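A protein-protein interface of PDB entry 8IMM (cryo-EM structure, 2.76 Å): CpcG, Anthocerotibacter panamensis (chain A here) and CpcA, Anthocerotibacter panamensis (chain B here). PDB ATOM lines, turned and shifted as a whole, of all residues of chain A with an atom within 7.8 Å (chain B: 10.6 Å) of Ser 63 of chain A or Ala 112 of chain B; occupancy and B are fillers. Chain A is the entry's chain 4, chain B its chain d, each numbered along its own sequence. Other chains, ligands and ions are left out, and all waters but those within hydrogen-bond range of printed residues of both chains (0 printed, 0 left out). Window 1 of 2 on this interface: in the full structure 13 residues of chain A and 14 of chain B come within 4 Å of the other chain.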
ATOM      1  N   LEU A  59     -26.880   2.135 -13.070  1.00  0.00           N
ATOM      2  CA  LEU A  59     -25.777   1.270 -13.425  1.00  0.00           C
ATOM      3  C   LEU A  59     -25.140   1.684 -14.735  1.00  0.00           C
ATOM      4  O   LEU A  59     -24.295   0.955 -15.257  1.00  0.00           O
ATOM      5  CB  LEU A  59     -26.246  -0.177 -13.510  1.00  0.00           C
ATOM      6  CG  LEU A  59     -27.018  -0.745 -12.324  1.00  0.00           C
ATOM      7  CD1 LEU A  59     -27.141  -2.235 -12.490  1.00  0.00           C
ATOM      8  CD2 LEU A  59     -26.338  -0.399 -11.020  1.00  0.00           C
ATOM      9  N   ILE A  60     -25.533   2.826 -15.287  1.00  0.00           N
ATOM     10  CA  ILE A  60     -24.879   3.337 -16.480  1.00  0.00           C
ATOM     11  C   ILE A  60     -23.620   4.051 -16.026  1.00  0.00           C
ATOM     12  O   ILE A  60     -23.619   5.263 -15.788  1.00  0.00           O
ATOM     13  CB  ILE A  60     -25.790   4.272 -17.288  1.00  0.00           C
ATOM     14  CG1 ILE A  60     -27.017   3.520 -17.771  1.00  0.00           C
ATOM     15  CG2 ILE A  60     -25.055   4.811 -18.492  1.00  0.00           C
ATOM     16  CD1 ILE A  60     -28.001   4.401 -18.466  1.00  0.00           C
ATOM     17  N   LEU A  61     -22.547   3.291 -15.895  1.00  0.00           N
ATOM     18  CA  LEU A  61     -21.244   3.786 -15.506  1.00  0.00           C
ATOM     19  C   LEU A  61     -20.245   3.322 -16.549  1.00  0.00           C
ATOM     20  O   LEU A  61     -20.485   2.344 -17.260  1.00  0.00           O
ATOM     21  CB  LEU A  61     -20.849   3.269 -14.128  1.00  0.00           C
ATOM     22  CG  LEU A  61     -21.190   4.060 -12.868  1.00  0.00           C
ATOM     23  CD1 LEU A  61     -22.641   4.424 -12.798  1.00  0.00           C
ATOM     24  CD2 LEU A  61     -20.827   3.222 -11.675  1.00  0.00           C
ATOM     25  N   GLU A  62     -19.123   4.030 -16.649  1.00  0.00           N
ATOM     26  CA  GLU A  62     -18.103   3.625 -17.604  1.00  0.00           C
ATOM     27  C   GLU A  62     -17.534   2.254 -17.280  1.00  0.00           C
ATOM     28  O   GLU A  62     -16.936   1.621 -18.154  1.00  0.00           O
ATOM     29  CB  GLU A  62     -16.981   4.658 -17.649  1.00  0.00           C
ATOM     30  CG  GLU A  62     -17.450   6.084 -17.870  1.00  0.00           C
ATOM     31  CD  GLU A  62     -17.688   6.417 -19.333  1.00  0.00           C
ATOM     32  OE1 GLU A  62     -17.507   7.595 -19.703  1.00  0.00           O
ATOM     33  OE2 GLU A  62     -18.058   5.513 -20.111  1.00  0.00           O
ATOM     34  N   SER A  63     -17.703   1.783 -16.044  1.00  0.00           N
ATOM     35  CA  SER A  63     -17.215   0.458 -15.689  1.00  0.00           C
ATOM     36  C   SER A  63     -18.222  -0.629 -16.035  1.00  0.00           C
ATOM     37  O   SER A  63     -17.837  -1.785 -16.225  1.00  0.00           O
ATOM     38  CB  SER A  63     -16.868   0.410 -14.209  1.00  0.00           C
ATOM     39  OG  SER A  63     -17.971   0.806 -13.423  1.00  0.00           O
ATOM     40  N   ASN A  64     -19.503  -0.288 -16.123  1.00  0.00           N
ATOM     41  CA  ASN A  64     -20.525  -1.267 -16.460  1.00  0.00           C
ATOM     42  C   ASN A  64     -20.787  -1.354 -17.952  1.00  0.00           C
ATOM     43  O   ASN A  64     -21.617  -2.160 -18.375  1.00  0.00           O
ATOM     44  CB  ASN A  64     -21.836  -0.933 -15.755  1.00  0.00           C
ATOM     45  CG  ASN A  64     -21.711  -0.978 -14.261  1.00  0.00           C
ATOM     46  OD1 ASN A  64     -21.054  -1.854 -13.712  1.00  0.00           O
ATOM     47  ND2 ASN A  64     -22.346  -0.037 -13.588  1.00  0.00           N
ATOM     48  N   ARG A  65     -20.100  -0.555 -18.751  1.00  0.00           N
ATOM     49  CA  ARG A  65     -20.429  -0.402 -20.157  1.00  0.00           C
ATOM     50  C   ARG A  65     -19.899  -1.593 -20.940  1.00  0.00           C
ATOM     51  O   ARG A  65     -18.709  -1.907 -20.871  1.00  0.00           O
ATOM     52  CB  ARG A  65     -19.840   0.903 -20.674  1.00  0.00           C
ATOM     53  CG  ARG A  65     -20.678   1.600 -21.705  1.00  0.00           C
ATOM     54  CD  ARG A  65     -19.915   2.740 -22.346  1.00  0.00           C
ATOM     55  NE  ARG A  65     -19.183   2.319 -23.536  1.00  0.00           N
ATOM     56  CZ  ARG A  65     -17.860   2.220 -23.598  1.00  0.00           C
ATOM     57  NH1 ARG A  65     -17.119   2.507 -22.535  1.00  0.00           N
ATOM     58  NH2 ARG A  65     -17.276   1.832 -24.724  1.00  0.00           N
ATOM     59  N   GLN A  66     -20.781  -2.250 -21.687  1.00  0.00           N
ATOM     60  CA  GLN A  66     -20.402  -3.382 -22.522  1.00  0.00           C
ATOM     61  C   GLN A  66     -19.877  -2.865 -23.852  1.00  0.00           C
ATOM     62  O   GLN A  66     -20.656  -2.520 -24.742  1.00  0.00           O
ATOM     63  CB  GLN A  66     -21.593  -4.307 -22.727  1.00  0.00           C
ATOM     64  CG  GLN A  66     -22.446  -4.453 -21.503  1.00  0.00           C
ATOM     65  CD  GLN A  66     -21.824  -5.370 -20.489  1.00  0.00           C
ATOM     66  OE1 GLN A  66     -21.116  -6.309 -20.839  1.00  0.00           O
ATOM     67  NE2 GLN A  66     -22.061  -5.092 -19.222  1.00  0.00           N
ATOM     68  N   THR A  67     -18.555  -2.823 -23.996  1.00  0.00           N
ATOM     69  CA  THR A  67     -17.952  -2.283 -25.206  1.00  0.00           C
ATOM     70  C   THR A  67     -18.148  -3.192 -26.411  1.00  0.00           C
ATOM     71  O   THR A  67     -18.457  -2.706 -27.505  1.00  0.00           O
ATOM     72  CB  THR A  67     -16.464  -2.058 -24.979  1.00  0.00           C
ATOM     73  OG1 THR A  67     -15.846  -3.313 -24.679  1.00  0.00           O
ATOM     74  CG2 THR A  67     -16.248  -1.126 -23.811  1.00  0.00           C
ATOM     75  N   VAL A  92     -22.052  -7.631 -14.905  1.00  0.00           N
ATOM     76  CA  VAL A  92     -22.655  -6.524 -14.175  1.00  0.00           C
ATOM     77  C   VAL A  92     -24.107  -6.818 -13.842  1.00  0.00           C
ATOM     78  O   VAL A  92     -24.554  -6.580 -12.716  1.00  0.00           O
ATOM     79  CB  VAL A  92     -22.506  -5.210 -14.953  1.00  0.00           C
ATOM     80  CG1 VAL A  92     -23.218  -5.284 -16.267  1.00  0.00           C
ATOM     81  CG2 VAL A  92     -23.122  -4.107 -14.153  1.00  0.00           C
ATOM     82  N   ARG A  95     -24.098  -9.432 -10.984  1.00  0.00           N
ATOM     83  CA  ARG A  95     -23.520  -8.941  -9.744  1.00  0.00           C
ATOM     84  C   ARG A  95     -24.348  -7.837  -9.120  1.00  0.00           C
ATOM     85  O   ARG A  95     -24.292  -7.645  -7.903  1.00  0.00           O
ATOM     86  CB  ARG A  95     -22.101  -8.439  -9.993  1.00  0.00           C
ATOM     87  CG  ARG A  95     -21.314  -8.232  -8.719  1.00  0.00           C
ATOM     88  CD  ARG A  95     -20.148  -7.282  -8.891  1.00  0.00           C
ATOM     89  NE  ARG A  95     -20.449  -6.149  -9.757  1.00  0.00           N
ATOM     90  CZ  ARG A  95     -19.957  -6.000 -10.983  1.00  0.00           C
ATOM     91  NH1 ARG A  95     -20.275  -4.935 -11.703  1.00  0.00           N
ATOM     92  NH2 ARG A  95     -19.144  -6.916 -11.487  1.00  0.00           N
ATOM     93  N   LEU A  96     -25.124  -7.110  -9.913  1.00  0.00           N
ATOM     94  CA  LEU A  96     -25.877  -5.994  -9.372  1.00  0.00           C
ATOM     95  C   LEU A  96     -27.349  -6.296  -9.168  1.00  0.00           C
ATOM     96  O   LEU A  96     -27.954  -5.730  -8.257  1.00  0.00           O
ATOM     97  CB  LEU A  96     -25.752  -4.775 -10.285  1.00  0.00           C
ATOM     98  CG  LEU A  96     -24.532  -3.864 -10.157  1.00  0.00           C
ATOM     99  CD1 LEU A  96     -24.502  -3.229  -8.795  1.00  0.00           C
ATOM    100  CD2 LEU A  96     -23.242  -4.586 -10.438  1.00  0.00           C
ATOM    101  N   ARG B   3     -15.608  -9.997  -5.445  1.00  0.00           N
ATOM    102  CA  ARG B   3     -15.329 -10.989  -6.472  1.00  0.00           C
ATOM    103  C   ARG B   3     -13.918 -11.515  -6.275  1.00  0.00           C
ATOM    104  O   ARG B   3     -12.954 -10.746  -6.312  1.00  0.00           O
ATOM    105  CB  ARG B   3     -15.508 -10.378  -7.865  1.00  0.00           C
ATOM    106  CG  ARG B   3     -15.377 -11.344  -9.013  1.00  0.00           C
ATOM    107  CD  ARG B   3     -13.943 -11.447  -9.462  1.00  0.00           C
ATOM    108  NE  ARG B   3     -13.390 -10.157  -9.851  1.00  0.00           N
ATOM    109  CZ  ARG B   3     -13.545  -9.611 -11.051  1.00  0.00           C
ATOM    110  NH1 ARG B   3     -14.234 -10.248 -11.985  1.00  0.00           N
ATOM    111  NH2 ARG B   3     -13.003  -8.431 -11.320  1.00  0.00           N
ATOM    112  N   TYR B  90      -6.908   3.712  -1.140  1.00  0.00           N
ATOM    113  CA  TYR B  90      -6.336   2.915  -2.222  1.00  0.00           C
ATOM    114  C   TYR B  90      -5.457   1.803  -1.676  1.00  0.00           C
ATOM    115  O   TYR B  90      -5.545   0.652  -2.122  1.00  0.00           O
ATOM    116  CB  TYR B  90      -5.536   3.805  -3.164  1.00  0.00           C
ATOM    117  CG  TYR B  90      -6.370   4.477  -4.212  1.00  0.00           C
ATOM    118  CD1 TYR B  90      -7.000   5.673  -3.952  1.00  0.00           C
ATOM    119  CD2 TYR B  90      -6.547   3.907  -5.449  1.00  0.00           C
ATOM    120  CE1 TYR B  90      -7.768   6.291  -4.895  1.00  0.00           C
ATOM    121  CE2 TYR B  90      -7.311   4.520  -6.403  1.00  0.00           C
ATOM    122  CZ  TYR B  90      -7.924   5.712  -6.118  1.00  0.00           C
ATOM    123  OH  TYR B  90      -8.696   6.337  -7.062  1.00  0.00           O
ATOM    124  N   PHE B  93      -7.593  -0.969  -0.041  1.00  0.00           N
ATOM    125  CA  PHE B  93      -8.273  -1.831  -0.993  1.00  0.00           C
ATOM    126  C   PHE B  93      -7.298  -2.692  -1.769  1.00  0.00           C
ATOM    127  O   PHE B  93      -7.657  -3.795  -2.188  1.00  0.00           O
ATOM    128  CB  PHE B  93      -9.122  -0.995  -1.933  1.00  0.00           C
ATOM    129  CG  PHE B  93     -10.293  -0.382  -1.263  1.00  0.00           C
ATOM    130  CD1 PHE B  93     -11.155  -1.161  -0.545  1.00  0.00           C
ATOM    131  CD2 PHE B  93     -10.518   0.967  -1.324  1.00  0.00           C
ATOM    132  CE1 PHE B  93     -12.217  -0.612   0.085  1.00  0.00           C
ATOM    133  CE2 PHE B  93     -11.585   1.523  -0.693  1.00  0.00           C
ATOM    134  CZ  PHE B  93     -12.435   0.734   0.011  1.00  0.00           C
ATOM    135  N   THR B 103      -9.324  -9.162  -7.902  1.00  0.00           N
ATOM    136  CA  THR B 103      -9.471  -7.716  -7.997  1.00  0.00           C
ATOM    137  C   THR B 103     -10.837  -7.251  -7.646  1.00  0.00           C
ATOM    138  O   THR B 103     -11.199  -6.141  -8.023  1.00  0.00           O
ATOM    139  CB  THR B 103      -9.116  -7.244  -9.403  1.00  0.00           C
ATOM    140  OG1 THR B 103      -9.905  -7.958 -10.357  1.00  0.00           O
ATOM    141  CG2 THR B 103      -7.653  -7.509  -9.684  1.00  0.00           C
ATOM    142  N   GLY B 104     -11.616  -8.068  -6.952  1.00  0.00           N
ATOM    143  CA  GLY B 104     -12.951  -7.703  -6.557  1.00  0.00           C
ATOM    144  C   GLY B 104     -13.032  -6.519  -5.621  1.00  0.00           C
ATOM    145  O   GLY B 104     -13.819  -5.602  -5.847  1.00  0.00           O
ATOM    146  N   PRO B 105     -12.250  -6.514  -4.538  1.00  0.00           N
ATOM    147  CA  PRO B 105     -12.289  -5.345  -3.649  1.00  0.00           C
ATOM    148  C   PRO B 105     -12.005  -4.043  -4.364  1.00  0.00           C
ATOM    149  O   PRO B 105     -12.759  -3.078  -4.206  1.00  0.00           O
ATOM    150  CB  PRO B 105     -11.225  -5.682  -2.608  1.00  0.00           C
ATOM    151  CG  PRO B 105     -11.277  -7.140  -2.532  1.00  0.00           C
ATOM    152  CD  PRO B 105     -11.528  -7.631  -3.915  1.00  0.00           C
ATOM    153  N   LEU B 106     -10.963  -4.000  -5.192  1.00  0.00           N
ATOM    154  CA  LEU B 106     -10.688  -2.790  -5.954  1.00  0.00           C
ATOM    155  C   LEU B 106     -11.820  -2.479  -6.918  1.00  0.00           C
ATOM    156  O   LEU B 106     -12.381  -1.383  -6.889  1.00  0.00           O
ATOM    157  CB  LEU B 106      -9.376  -2.930  -6.715  1.00  0.00           C
ATOM    158  CG  LEU B 106      -8.106  -2.452  -6.034  1.00  0.00           C
ATOM    159  CD1 LEU B 106      -6.919  -2.967  -6.798  1.00  0.00           C
ATOM    160  CD2 LEU B 106      -8.101  -0.949  -5.989  1.00  0.00           C
ATOM    161  N   ASP B 107     -12.201  -3.449  -7.747  1.00  0.00           N
ATOM    162  CA  ASP B 107     -13.170  -3.183  -8.801  1.00  0.00           C
ATOM    163  C   ASP B 107     -14.502  -2.721  -8.233  1.00  0.00           C
ATOM    164  O   ASP B 107     -15.161  -1.860  -8.820  1.00  0.00           O
ATOM    165  CB  ASP B 107     -13.346  -4.437  -9.658  1.00  0.00           C
ATOM    166  CG  ASP B 107     -14.455  -4.307 -10.692  1.00  0.00           C
ATOM    167  OD1 ASP B 107     -14.785  -3.175 -11.105  1.00  0.00           O
ATOM    168  OD2 ASP B 107     -15.009  -5.353 -11.093  1.00  0.00           O
ATOM    169  N   ASP B 108     -14.905  -3.252  -7.086  1.00  0.00           N
ATOM    170  CA  ASP B 108     -16.185  -2.891  -6.495  1.00  0.00           C
ATOM    171  C   ASP B 108     -16.124  -1.625  -5.652  1.00  0.00           C
ATOM    172  O   ASP B 108     -17.101  -0.874  -5.606  1.00  0.00           O
ATOM    173  CB  ASP B 108     -16.723  -4.047  -5.652  1.00  0.00           C
ATOM    174  CG  ASP B 108     -17.108  -5.247  -6.490  1.00  0.00           C
ATOM    175  OD1 ASP B 108     -16.210  -5.995  -6.926  1.00  0.00           O
ATOM    176  OD2 ASP B 108     -18.319  -5.439  -6.725  1.00  0.00           O
ATOM    177  N   TYR B 109     -15.008  -1.357  -4.978  1.00  0.00           N
ATOM    178  CA  TYR B 109     -15.007  -0.204  -4.093  1.00  0.00           C
ATOM    179  C   TYR B 109     -14.436   1.035  -4.767  1.00  0.00           C
ATOM    180  O   TYR B 109     -15.041   2.108  -4.694  1.00  0.00           O
ATOM    181  CB  TYR B 109     -14.247  -0.537  -2.818  1.00  0.00           C
ATOM    182  CG  TYR B 109     -15.022  -1.444  -1.894  1.00  0.00           C
ATOM    183  CD1 TYR B 109     -15.979  -0.939  -1.037  1.00  0.00           C
ATOM    184  CD2 TYR B 109     -14.791  -2.805  -1.880  1.00  0.00           C
ATOM    185  CE1 TYR B 109     -16.681  -1.765  -0.200  1.00  0.00           C
ATOM    186  CE2 TYR B 109     -15.486  -3.635  -1.048  1.00  0.00           C
ATOM    187  CZ  TYR B 109     -16.429  -3.114  -0.210  1.00  0.00           C
ATOM    188  OH  TYR B 109     -17.126  -3.953   0.624  1.00  0.00           O
ATOM    189  N   VAL B 110     -13.296   0.920  -5.438  1.00  0.00           N
ATOM    190  CA  VAL B 110     -12.662   2.084  -6.036  1.00  0.00           C
ATOM    191  C   VAL B 110     -13.141   2.272  -7.467  1.00  0.00           C
ATOM    192  O   VAL B 110     -13.757   3.289  -7.796  1.00  0.00           O
ATOM    193  CB  VAL B 110     -11.132   1.962  -5.997  1.00  0.00           C
ATOM    194  CG1 VAL B 110     -10.502   3.026  -6.854  1.00  0.00           C
ATOM    195  CG2 VAL B 110     -10.629   2.072  -4.587  1.00  0.00           C
ATOM    196  N   ILE B 111     -12.875   1.287  -8.323  1.00  0.00           N
ATOM    197  CA  ILE B 111     -12.990   1.498  -9.760  1.00  0.00           C
ATOM    198  C   ILE B 111     -14.418   1.790 -10.184  1.00  0.00           C
ATOM    199  O   ILE B 111     -14.652   2.693 -10.993  1.00  0.00           O
ATOM    200  CB  ILE B 111     -12.427   0.286 -10.514  1.00  0.00           C
ATOM    201  CG1 ILE B 111     -10.938   0.139 -10.235  1.00  0.00           C
ATOM    202  CG2 ILE B 111     -12.655   0.435 -11.986  1.00  0.00           C
ATOM    203  CD1 ILE B 111     -10.391  -1.197 -10.624  1.00  0.00           C
ATOM    204  N   ALA B 112     -15.393   1.049  -9.668  1.00  0.00           N
ATOM    205  CA  ALA B 112     -16.769   1.189 -10.134  1.00  0.00           C
ATOM    206  C   ALA B 112     -17.315   2.545  -9.720  1.00  0.00           C
ATOM    207  O   ALA B 112     -17.670   2.747  -8.558  1.00  0.00           O
ATOM    208  CB  ALA B 112     -17.634   0.067  -9.579  1.00  0.00           C
ATOM    209  N   GLY B 113     -17.412   3.465 -10.672  1.00  0.00           N
ATOM    210  CA  GLY B 113     -17.769   4.831 -10.368  1.00  0.00           C
ATOM    211  C   GLY B 113     -16.604   5.777 -10.242  1.00  0.00           C
ATOM    212  O   GLY B 113     -16.769   6.867  -9.687  1.00  0.00           O
ATOM    213  N   LEU B 114     -15.426   5.397 -10.727  1.00  0.00           N
ATOM    214  CA  LEU B 114     -14.241   6.228 -10.553  1.00  0.00           C
ATOM    215  C   LEU B 114     -14.297   7.461 -11.437  1.00  0.00           C
ATOM    216  O   LEU B 114     -14.055   8.581 -10.975  1.00  0.00           O
ATOM    217  CB  LEU B 114     -12.999   5.406 -10.863  1.00  0.00           C
ATOM    218  CG  LEU B 114     -11.620   5.970 -10.576  1.00  0.00           C
ATOM    219  CD1 LEU B 114     -11.512   6.393  -9.143  1.00  0.00           C
ATOM    220  CD2 LEU B 114     -10.612   4.908 -10.887  1.00  0.00           C
ATOM    221  N   ARG B 115     -14.621   7.274 -12.715  1.00  0.00           N
ATOM    222  CA  ARG B 115     -14.618   8.389 -13.650  1.00  0.00           C
ATOM    223  C   ARG B 115     -15.701   9.395 -13.309  1.00  0.00           C
ATOM    224  O   ARG B 115     -15.462  10.604 -13.335  1.00  0.00           O
ATOM    225  CB  ARG B 115     -14.800   7.872 -15.067  1.00  0.00           C
ATOM    226  CG  ARG B 115     -13.645   7.039 -15.542  1.00  0.00           C
ATOM    227  CD  ARG B 115     -13.591   6.967 -17.056  1.00  0.00           C
ATOM    228  NE  ARG B 115     -13.026   5.719 -17.575  1.00  0.00           N
ATOM    229  CZ  ARG B 115     -11.878   5.162 -17.194  1.00  0.00           C
ATOM    230  NH1 ARG B 115     -11.090   5.739 -16.297  1.00  0.00           N
ATOM    231  NH2 ARG B 115     -11.493   4.023 -17.750  1.00  0.00           N
ATOM    232  N   GLU B 116     -16.899   8.915 -12.985  1.00  0.00           N
ATOM    233  CA  GLU B 116     -18.003   9.815 -12.681  1.00  0.00           C
ATOM    234  C   GLU B 116     -17.691  10.680 -11.473  1.00  0.00           C
ATOM    235  O   GLU B 116     -17.912  11.895 -11.495  1.00  0.00           O
ATOM    236  CB  GLU B 116     -19.270   9.003 -12.438  1.00  0.00           C
ATOM    237  CG  GLU B 116     -19.951   8.514 -13.698  1.00  0.00           C
ATOM    238  CD  GLU B 116     -19.255   7.330 -14.337  1.00  0.00           C
ATOM    239  OE1 GLU B 116     -19.839   6.736 -15.266  1.00  0.00           O
ATOM    240  OE2 GLU B 116     -18.132   6.983 -13.919  1.00  0.00           O
ATOM    241  N   VAL B 117     -17.162  10.076 -10.413  1.00  0.00           N
ATOM    242  CA  VAL B 117     -16.867  10.829  -9.203  1.00  0.00           C
ATOM    243  C   VAL B 117     -15.700  11.777  -9.427  1.00  0.00           C
ATOM    244  O   VAL B 117     -15.742  12.939  -9.012  1.00  0.00           O
ATOM    245  CB  VAL B 117     -16.598   9.872  -8.038  1.00  0.00           C
ATOM    246  CG1 VAL B 117     -16.119  10.645  -6.853  1.00  0.00           C
ATOM    247  CG2 VAL B 117     -17.849   9.126  -7.697  1.00  0.00           C
ATOM    248  N   ASN B 118     -14.641  11.305 -10.083  1.00  0.00           N
ATOM    249  CA  ASN B 118     -13.491  12.167 -10.323  1.00  0.00           C
ATOM    250  C   ASN B 118     -13.860  13.345 -11.210  1.00  0.00           C
ATOM    251  O   ASN B 118     -13.359  14.456 -11.019  1.00  0.00           O
ATOM    252  CB  ASN B 118     -12.359  11.361 -10.942  1.00  0.00           C
ATOM    253  CG  ASN B 118     -11.579  10.591  -9.919  1.00  0.00           C
ATOM    254  OD1 ASN B 118     -11.854  10.672  -8.727  1.00  0.00           O
ATOM    255  ND2 ASN B 118     -10.608   9.824 -10.373  1.00  0.00           N
ATOM    256  N   ARG B 119     -14.735  13.123 -12.186  1.00  0.00           N
ATOM    257  CA  ARG B 119     -15.182  14.203 -13.049  1.00  0.00           C
ATOM    258  C   ARG B 119     -16.100  15.164 -12.317  1.00  0.00           C
ATOM    259  O   ARG B 119     -16.066  16.368 -12.580  1.00  0.00           O
ATOM    260  CB  ARG B 119     -15.885  13.618 -14.262  1.00  0.00           C
ATOM    261  CG  ARG B 119     -16.108  14.582 -15.384  1.00  0.00           C
ATOM    262  CD  ARG B 119     -17.365  14.234 -16.173  1.00  0.00           C
ATOM    263  NE  ARG B 119     -17.582  12.796 -16.349  1.00  0.00           N
ATOM    264  CZ  ARG B 119     -16.749  11.960 -16.964  1.00  0.00           C
ATOM    265  NH1 ARG B 119     -15.604  12.393 -17.470  1.00  0.00           N
ATOM    266  NH2 ARG B 119     -17.061  10.675 -17.065  1.00  0.00           N
ATOM    267  N   HIS B 157      -2.992  -2.979 -11.636  1.00  0.00           N
ATOM    268  CA  HIS B 157      -4.391  -2.975 -12.041  1.00  0.00           C
ATOM    269  C   HIS B 157      -5.063  -1.664 -11.668  1.00  0.00           C
ATOM    270  O   HIS B 157      -5.832  -1.105 -12.458  1.00  0.00           O
ATOM    271  CB  HIS B 157      -5.134  -4.147 -11.415  1.00  0.00           C
ATOM    272  CG  HIS B 157      -6.606  -4.118 -11.664  1.00  0.00           C
ATOM    273  ND1 HIS B 157      -7.155  -4.394 -12.896  1.00  0.00           N
ATOM    274  CD2 HIS B 157      -7.644  -3.842 -10.843  1.00  0.00           C
ATOM    275  CE1 HIS B 157      -8.469  -4.288 -12.823  1.00  0.00           C
ATOM    276  NE2 HIS B 157      -8.791  -3.956 -11.587  1.00  0.00           N
ATOM    277  N   ALA B 158      -4.779  -1.151 -10.472  1.00  0.00           N
ATOM    278  CA  ALA B 158      -5.360   0.130 -10.082  1.00  0.00           C
ATOM    279  C   ALA B 158      -4.892   1.255 -10.999  1.00  0.00           C
ATOM    280  O   ALA B 158      -5.690   2.112 -11.404  1.00  0.00           O
ATOM    281  CB  ALA B 158      -5.019   0.446  -8.633  1.00  0.00           C
ATOM    282  N   ALA B 161      -6.624   1.078 -14.233  1.00  0.00           N
ATOM    283  CA  ALA B 161      -8.006   1.512 -14.092  1.00  0.00           C
ATOM    284  C   ALA B 161      -8.114   3.027 -14.096  1.00  0.00           C
ATOM    285  O   ALA B 161      -9.002   3.590 -14.743  1.00  0.00           O
ATOM    286  CB  ALA B 161      -8.605   0.942 -12.812  1.00  0.00           C
ATOM    287  N   LEU B 162      -7.222   3.706 -13.374  1.00  0.00           N
ATOM    288  CA  LEU B 162      -7.281   5.164 -13.310  1.00  0.00           C
ATOM    289  C   LEU B 162      -7.010   5.797 -14.667  1.00  0.00           C
ATOM    290  O   LEU B 162      -7.685   6.753 -15.062  1.00  0.00           O
ATOM    291  CB  LEU B 162      -6.287   5.681 -12.279  1.00  0.00           C
ATOM    292  CG  LEU B 162      -6.796   5.729 -10.853  1.00  0.00           C
ATOM    293  CD1 LEU B 162      -5.648   5.582  -9.898  1.00  0.00           C
ATOM    294  CD2 LEU B 162      -7.490   7.048 -10.643  1.00  0.00           C
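N of Glu 62 of chain A is in hydrogen-bond range of OE1 of Glu 116 of chain B (3.1 Å). The guanidinium group (NE) of Arg 95 of chain A lies within salt-bridge range of the side-chain carboxylate (OD2) of Asp 108 of chain B, at 3.8 Å.
The backbone carbonyl oxygen (O) of Gly 104 of chain B sits close to the side-chain carboxylate (OD1) of Asp 108 of chain B (2.7 Å). NH1 of Arg 65 of chain A is in salt-bridge range of OE2 of Glu 62 of chain A, 3.97 Å away. O of Asp 107 of chain B sits at hydrogen-bond distance from N of Ala 112 of chain B (3.0 Å).
N of Gly 113 of chain B touches CD2 of Leu 61 of chain A, 3.6 Å away. OE1 of Glu 116 of chain B touches CA of Leu 61 of chain A, at 3.3 Å. Ala 112 of chain B touches Ser 63 of chain A. OG of Ser 63 of chain A touches N of Gly 113 of chain B, at 3.9 Å.
Of the printed residues of chain B, Glu 62 of chain A touches Glu 116 (3.1 Å). Printed residues of chain B within 4 Å of Ser 63 of chain A: Ala 112 (3.5 Å) and Gly 113 (3.9 Å). Asn 64 of chain A touches none of the printed residues of chain B. Gln 66 of chain A touches none of the printed residues of chain B. Printed residues of chain B within 4 Å of Arg 95 of chain A: Asp 108. Of chain A, only Ser 63 comes within 4 Å of Ala 112 of chain B. Arg 115 of chain B touches none of the printed residues of chain A. Printed residues of chain A within 4 Å of Glu 116 of chain B: Leu 61 (3.3 Å) and Glu 62 (3.1 Å). The nearest residue of chain B that does not touch Ser 63 of chain A is Ile 111 of chain B (4.5 Å). The nearest printed residue of chain A that does not touch Asp 108 of chain B is Leu 96 of chain A (6.2 Å).
Of the 24 printed residues of chain B, 4 touch a printed residue of chain A. Printed residues of chain B that touch a printed residue of chain A: Asp 108, Ala 112, Gly 113 and Glu 116. Hydrophobic or aromatic side chains of chain B within 4 Å of the printed part of chain A: Ala 112. Hydrophobic or aromatic side chains of chain A within 4 Å of the printed part of chain B: Leu 61. Among the printed residues, 6 pairs touch across the chains. Among the printed residues, Asp or Glu carboxylates within 4 Å of a Lys or Arg side-chain nitrogen of the other chain: Arg 95 of chain A with Asp 108 of chain B.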
